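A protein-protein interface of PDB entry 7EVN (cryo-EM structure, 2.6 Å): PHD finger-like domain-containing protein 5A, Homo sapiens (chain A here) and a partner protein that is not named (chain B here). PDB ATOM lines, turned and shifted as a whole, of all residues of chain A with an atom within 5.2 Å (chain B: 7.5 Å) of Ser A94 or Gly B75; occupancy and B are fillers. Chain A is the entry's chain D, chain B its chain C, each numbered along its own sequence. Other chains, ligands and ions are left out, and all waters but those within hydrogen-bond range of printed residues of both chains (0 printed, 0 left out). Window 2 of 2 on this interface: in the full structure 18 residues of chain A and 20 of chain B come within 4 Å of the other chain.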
ATOM      1  N   ASN A  90      -7.242 -10.589 -31.339  1.00  0.00           N
ATOM      2  CA  ASN A  90      -8.444 -11.397 -31.496  1.00  0.00           C
ATOM      3  C   ASN A  90      -9.581 -10.479 -31.924  1.00  0.00           C
ATOM      4  O   ASN A  90     -10.076  -9.677 -31.127  1.00  0.00           O
ATOM      5  CB  ASN A  90      -8.785 -12.131 -30.203  1.00  0.00           C
ATOM      6  CG  ASN A  90      -9.733 -13.292 -30.424  1.00  0.00           C
ATOM      7  OD1 ASN A  90     -10.480 -13.326 -31.400  1.00  0.00           O
ATOM      8  ND2 ASN A  90      -9.709 -14.252 -29.512  1.00  0.00           N
ATOM      9  N   GLY A  92     -12.556 -11.627 -33.106  1.00  0.00           N
ATOM     10  CA  GLY A  92     -13.847 -12.245 -32.894  1.00  0.00           C
ATOM     11  C   GLY A  92     -14.435 -11.944 -31.534  1.00  0.00           C
ATOM     12  O   GLY A  92     -15.625 -12.171 -31.298  1.00  0.00           O
ATOM     13  N   SER A  93     -13.604 -11.442 -30.627  1.00  0.00           N
ATOM     14  CA  SER A  93     -14.044 -11.103 -29.287  1.00  0.00           C
ATOM     15  C   SER A  93     -13.700  -9.648 -28.971  1.00  0.00           C
ATOM     16  O   SER A  93     -13.265  -8.881 -29.833  1.00  0.00           O
ATOM     17  CB  SER A  93     -13.431 -12.068 -28.275  1.00  0.00           C
ATOM     18  OG  SER A  93     -13.994 -13.360 -28.404  1.00  0.00           O
ATOM     19  N   SER A  94     -13.901  -9.259 -27.715  1.00  0.00           N
ATOM     20  CA  SER A  94     -13.703  -7.893 -27.253  1.00  0.00           C
ATOM     21  C   SER A  94     -12.425  -7.795 -26.423  1.00  0.00           C
ATOM     22  O   SER A  94     -11.637  -8.741 -26.334  1.00  0.00           O
ATOM     23  CB  SER A  94     -14.922  -7.411 -26.461  1.00  0.00           C
ATOM     24  OG  SER A  94     -16.124  -7.904 -27.024  1.00  0.00           O
ATOM     25  N   LYS A  95     -12.218  -6.618 -25.822  1.00  0.00           N
ATOM     26  CA  LYS A  95     -10.983  -6.356 -25.087  1.00  0.00           C
ATOM     27  C   LYS A  95     -10.837  -7.276 -23.881  1.00  0.00           C
ATOM     28  O   LYS A  95      -9.882  -8.060 -23.805  1.00  0.00           O
ATOM     29  CB  LYS A  95     -10.936  -4.893 -24.646  1.00  0.00           C
ATOM     30  CG  LYS A  95     -10.297  -3.958 -25.658  1.00  0.00           C
ATOM     31  CD  LYS A  95      -9.381  -2.947 -24.990  1.00  0.00           C
ATOM     32  CE  LYS A  95      -8.000  -3.528 -24.743  1.00  0.00           C
ATOM     33  NZ  LYS A  95      -7.134  -3.473 -25.954  1.00  0.00           N
ATOM     34  N   THR A  96     -11.770  -7.202 -22.928  1.00  0.00           N
ATOM     35  CA  THR A  96     -11.672  -8.033 -21.733  1.00  0.00           C
ATOM     36  C   THR A  96     -12.115  -9.470 -21.975  1.00  0.00           C
ATOM     37  O   THR A  96     -12.313 -10.210 -21.004  1.00  0.00           O
ATOM     38  CB  THR A  96     -12.491  -7.436 -20.585  1.00  0.00           C
ATOM     39  OG1 THR A  96     -12.458  -8.328 -19.466  1.00  0.00           O
ATOM     40  CG2 THR A  96     -13.940  -7.235 -21.010  1.00  0.00           C
ATOM     41  N   ASP A  97     -12.293  -9.875 -23.228  1.00  0.00           N
ATOM     42  CA  ASP A  97     -12.622 -11.255 -23.543  1.00  0.00           C
ATOM     43  C   ASP A  97     -11.351 -12.102 -23.612  1.00  0.00           C
ATOM     44  O   ASP A  97     -10.268 -11.696 -23.179  1.00  0.00           O
ATOM     45  CB  ASP A  97     -13.405 -11.327 -24.850  1.00  0.00           C
ATOM     46  CG  ASP A  97     -14.905 -11.217 -24.642  1.00  0.00           C
ATOM     47  OD1 ASP A  97     -15.588 -12.263 -24.680  1.00  0.00           O
ATOM     48  OD2 ASP A  97     -15.401 -10.089 -24.440  1.00  0.00           O
ATOM     49  N   LEU A  98     -11.495 -13.310 -24.148  1.00  0.00           N
ATOM     50  CA  LEU A  98     -10.360 -14.204 -24.355  1.00  0.00           C
ATOM     51  C   LEU A  98      -9.309 -13.566 -25.260  1.00  0.00           C
ATOM     52  O   LEU A  98      -9.591 -12.610 -25.984  1.00  0.00           O
ATOM     53  CB  LEU A  98     -10.819 -15.535 -24.957  1.00  0.00           C
ATOM     54  CG  LEU A  98     -11.488 -15.477 -26.334  1.00  0.00           C
ATOM     55  CD1 LEU A  98     -11.047 -16.648 -27.198  1.00  0.00           C
ATOM     56  CD2 LEU A  98     -12.997 -15.465 -26.196  1.00  0.00           C
ATOM     57  N   LEU B  69     -21.886   5.097 -27.063  1.00  0.00           N
ATOM     58  CA  LEU B  69     -20.990   4.836 -25.939  1.00  0.00           C
ATOM     59  C   LEU B  69     -21.027   3.370 -25.526  1.00  0.00           C
ATOM     60  O   LEU B  69     -19.983   2.765 -25.258  1.00  0.00           O
ATOM     61  CB  LEU B  69     -21.358   5.728 -24.755  1.00  0.00           C
ATOM     62  CG  LEU B  69     -20.979   7.204 -24.865  1.00  0.00           C
ATOM     63  CD1 LEU B  69     -21.322   7.918 -23.579  1.00  0.00           C
ATOM     64  CD2 LEU B  69     -19.509   7.365 -25.192  1.00  0.00           C
ATOM     65  N   LEU B  70     -22.225   2.791 -25.429  1.00  0.00           N
ATOM     66  CA  LEU B  70     -22.328   1.362 -25.155  1.00  0.00           C
ATOM     67  C   LEU B  70     -21.663   0.548 -26.252  1.00  0.00           C
ATOM     68  O   LEU B  70     -21.002  -0.459 -25.970  1.00  0.00           O
ATOM     69  CB  LEU B  70     -23.798   0.969 -25.007  1.00  0.00           C
ATOM     70  CG  LEU B  70     -24.169  -0.322 -24.272  1.00  0.00           C
ATOM     71  CD1 LEU B  70     -24.047  -1.549 -25.166  1.00  0.00           C
ATOM     72  CD2 LEU B  70     -23.343  -0.491 -23.015  1.00  0.00           C
ATOM     73  N   LYS B  71     -21.826   0.979 -27.504  1.00  0.00           N
ATOM     74  CA  LYS B  71     -21.128   0.337 -28.616  1.00  0.00           C
ATOM     75  C   LYS B  71     -19.613   0.393 -28.438  1.00  0.00           C
ATOM     76  O   LYS B  71     -18.913  -0.579 -28.740  1.00  0.00           O
ATOM     77  CB  LYS B  71     -21.524   1.016 -29.923  1.00  0.00           C
ATOM     78  CG  LYS B  71     -21.748   0.101 -31.099  1.00  0.00           C
ATOM     79  CD  LYS B  71     -22.513   0.851 -32.175  1.00  0.00           C
ATOM     80  CE  LYS B  71     -22.803  -0.025 -33.375  1.00  0.00           C
ATOM     81  NZ  LYS B  71     -23.732   0.644 -34.326  1.00  0.00           N
ATOM     82  N   ILE B  72     -19.097   1.523 -27.956  1.00  0.00           N
ATOM     83  CA  ILE B  72     -17.661   1.704 -27.772  1.00  0.00           C
ATOM     84  C   ILE B  72     -17.146   0.848 -26.625  1.00  0.00           C
ATOM     85  O   ILE B  72     -16.063   0.263 -26.708  1.00  0.00           O
ATOM     86  CB  ILE B  72     -17.348   3.196 -27.541  1.00  0.00           C
ATOM     87  CG1 ILE B  72     -17.394   3.969 -28.854  1.00  0.00           C
ATOM     88  CG2 ILE B  72     -15.996   3.367 -26.882  1.00  0.00           C
ATOM     89  CD1 ILE B  72     -17.603   5.449 -28.677  1.00  0.00           C
ATOM     90  N   LYS B  73     -17.907   0.765 -25.537  1.00  0.00           N
ATOM     91  CA  LYS B  73     -17.427   0.051 -24.359  1.00  0.00           C
ATOM     92  C   LYS B  73     -17.520  -1.458 -24.549  1.00  0.00           C
ATOM     93  O   LYS B  73     -16.546  -2.182 -24.320  1.00  0.00           O
ATOM     94  CB  LYS B  73     -18.208   0.492 -23.122  1.00  0.00           C
ATOM     95  CG  LYS B  73     -18.010  -0.413 -21.930  1.00  0.00           C
ATOM     96  CD  LYS B  73     -18.377   0.280 -20.636  1.00  0.00           C
ATOM     97  CE  LYS B  73     -18.775  -0.731 -19.575  1.00  0.00           C
ATOM     98  NZ  LYS B  73     -20.093  -1.360 -19.867  1.00  0.00           N
ATOM     99  N   ASN B  74     -18.684  -1.957 -24.968  1.00  0.00           N
ATOM    100  CA  ASN B  74     -18.887  -3.396 -25.150  1.00  0.00           C
ATOM    101  C   ASN B  74     -18.999  -3.688 -26.642  1.00  0.00           C
ATOM    102  O   ASN B  74     -20.078  -3.663 -27.232  1.00  0.00           O
ATOM    103  CB  ASN B  74     -20.123  -3.870 -24.393  1.00  0.00           C
ATOM    104  CG  ASN B  74     -20.093  -3.492 -22.935  1.00  0.00           C
ATOM    105  OD1 ASN B  74     -20.543  -2.414 -22.552  1.00  0.00           O
ATOM    106  ND2 ASN B  74     -19.562  -4.379 -22.106  1.00  0.00           N
ATOM    107  N   GLY B  75     -17.859  -3.972 -27.259  1.00  0.00           N
ATOM    108  CA  GLY B  75     -17.840  -4.277 -28.675  1.00  0.00           C
ATOM    109  C   GLY B  75     -16.475  -4.742 -29.125  1.00  0.00           C
ATOM    110  O   GLY B  75     -15.471  -4.579 -28.424  1.00  0.00           O
ATOM    111  N   THR B  76     -16.453  -5.325 -30.319  1.00  0.00           N
ATOM    112  CA  THR B  76     -15.216  -5.788 -30.912  1.00  0.00           C
ATOM    113  C   THR B  76     -14.413  -4.596 -31.434  1.00  0.00           C
ATOM    114  O   THR B  76     -14.919  -3.475 -31.479  1.00  0.00           O
ATOM    115  CB  THR B  76     -15.519  -6.772 -32.037  1.00  0.00           C
ATOM    116  OG1 THR B  76     -16.554  -6.242 -32.871  1.00  0.00           O
ATOM    117  CG2 THR B  76     -15.976  -8.096 -31.460  1.00  0.00           C
ATOM    118  N   PRO B  77     -13.149  -4.806 -31.799  1.00  0.00           N
ATOM    119  CA  PRO B  77     -12.332  -3.705 -32.326  1.00  0.00           C
ATOM    120  C   PRO B  77     -12.978  -2.985 -33.500  1.00  0.00           C
ATOM    121  O   PRO B  77     -12.939  -1.746 -33.544  1.00  0.00           O
ATOM    122  CB  PRO B  77     -11.030  -4.407 -32.734  1.00  0.00           C
ATOM    123  CG  PRO B  77     -10.911  -5.506 -31.754  1.00  0.00           C
ATOM    124  CD  PRO B  77     -12.312  -5.960 -31.421  1.00  0.00           C
ATOM    125  N   PRO B  78     -13.565  -3.692 -34.483  1.00  0.00           N
ATOM    126  CA  PRO B  78     -14.181  -2.953 -35.604  1.00  0.00           C
ATOM    127  C   PRO B  78     -15.346  -2.073 -35.183  1.00  0.00           C
ATOM    128  O   PRO B  78     -15.427  -0.905 -35.598  1.00  0.00           O
ATOM    129  CB  PRO B  78     -14.622  -4.072 -36.555  1.00  0.00           C
ATOM    130  CG  PRO B  78     -13.764  -5.217 -36.210  1.00  0.00           C
ATOM    131  CD  PRO B  78     -13.618  -5.143 -34.734  1.00  0.00           C
ATOM    132  N   MET B  79     -16.262  -2.607 -34.374  1.00  0.00           N
ATOM    133  CA  MET B  79     -17.371  -1.802 -33.879  1.00  0.00           C
ATOM    134  C   MET B  79     -16.870  -0.623 -33.059  1.00  0.00           C
ATOM    135  O   MET B  79     -17.407   0.487 -33.161  1.00  0.00           O
ATOM    136  CB  MET B  79     -18.319  -2.668 -33.051  1.00  0.00           C
ATOM    137  CG  MET B  79     -18.918  -3.832 -33.816  1.00  0.00           C
ATOM    138  SD  MET B  79     -19.468  -5.174 -32.747  1.00  0.00           S
ATOM    139  CE  MET B  79     -20.363  -4.269 -31.492  1.00  0.00           C
ATOM    140  N   ARG B  80     -15.835  -0.842 -32.246  1.00  0.00           N
ATOM    141  CA  ARG B  80     -15.281   0.232 -31.433  1.00  0.00           C
ATOM    142  C   ARG B  80     -14.724   1.346 -32.305  1.00  0.00           C
ATOM    143  O   ARG B  80     -14.990   2.526 -32.065  1.00  0.00           O
ATOM    144  CB  ARG B  80     -14.200  -0.317 -30.503  1.00  0.00           C
ATOM    145  CG  ARG B  80     -14.744  -1.088 -29.317  1.00  0.00           C
ATOM    146  CD  ARG B  80     -13.736  -1.148 -28.182  1.00  0.00           C
ATOM    147  NE  ARG B  80     -12.944  -2.371 -28.222  1.00  0.00           N
ATOM    148  CZ  ARG B  80     -11.738  -2.456 -28.768  1.00  0.00           C
ATOM    149  NH1 ARG B  80     -11.183  -1.386 -29.317  1.00  0.00           N
ATOM    150  NH2 ARG B  80     -11.087  -3.607 -28.766  1.00  0.00           N
ATOM    151  N   GLN B 115      -9.621  -1.314 -18.473  1.00  0.00           N
ATOM    152  CA  GLN B 115      -9.633  -1.182 -19.924  1.00  0.00           C
ATOM    153  C   GLN B 115     -10.785  -0.309 -20.405  1.00  0.00           C
ATOM    154  O   GLN B 115     -10.609   0.497 -21.329  1.00  0.00           O
ATOM    155  CB  GLN B 115      -9.696  -2.563 -20.564  1.00  0.00           C
ATOM    156  CG  GLN B 115      -8.908  -3.602 -19.797  1.00  0.00           C
ATOM    157  CD  GLN B 115      -9.471  -4.993 -19.964  1.00  0.00           C
ATOM    158  OE1 GLN B 115      -9.649  -5.724 -18.990  1.00  0.00           O
ATOM    159  NE2 GLN B 115      -9.755  -5.369 -21.205  1.00  0.00           N
ATOM    160  N   LEU B 119     -10.555   3.204 -22.519  1.00  0.00           N
ATOM    161  CA  LEU B 119     -11.362   3.526 -23.694  1.00  0.00           C
ATOM    162  C   LEU B 119     -12.135   4.826 -23.504  1.00  0.00           C
ATOM    163  O   LEU B 119     -12.234   5.646 -24.427  1.00  0.00           O
ATOM    164  CB  LEU B 119     -12.323   2.379 -23.992  1.00  0.00           C
ATOM    165  CG  LEU B 119     -11.678   1.081 -24.462  1.00  0.00           C
ATOM    166  CD1 LEU B 119     -12.632  -0.084 -24.301  1.00  0.00           C
ATOM    167  CD2 LEU B 119     -11.243   1.223 -25.900  1.00  0.00           C
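Of chain B, only Gly B75 (3.5 Å) comes within 4 Å of Ser A94.
Of chain A, only Ser A94 comes within 4 Å of Gly B75.
Of the printed residues of chain B, Thr A96 touches Gln B115.
Of the printed residues of chain A, Pro B77 touches Ser A93 (3.5 Å).
Of the printed residues of chain A, Thr B76 touches Ser A93.
The nearest residue of chain B that does not touch Ser A94 is Thr B76 (4.2 Å).
The nearest residue of chain A that does not touch Gly B75 is Lys A95 (4.6 Å).
The nearest printed residue of chain A that does not touch Arg B80 is Ser A94 (5.0 Å).
SD of Met B79 lies within hydrogen-bond range of OG1 of Thr B76.
The backbone carbonyl oxygen of Gly B75 lies within hydrogen-bond range of the guanidinium group of Arg B80, at 3.4 Å.
OG of Ser A94 sits close to OD2 of Asp A97 (3.5 Å).
Among the printed residues, no Asp or Glu carboxylate lies within 4 Å of a Lys or Arg side-chain nitrogen of the other chain.
NE2 of Gln B115 lies close to N of Thr A96, 3.2 Å away.
O of Ser A93 touches CG2 of Thr B76, 3.3 Å away.
Ser A93 touches Pro B77.
Gly B75 touches Ser A94 (O to CB, 3.5 Å).
Arg B80 touches Lys A95.
Lys A95 touches Gln B115 (C to NE2, 3.5 Å).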
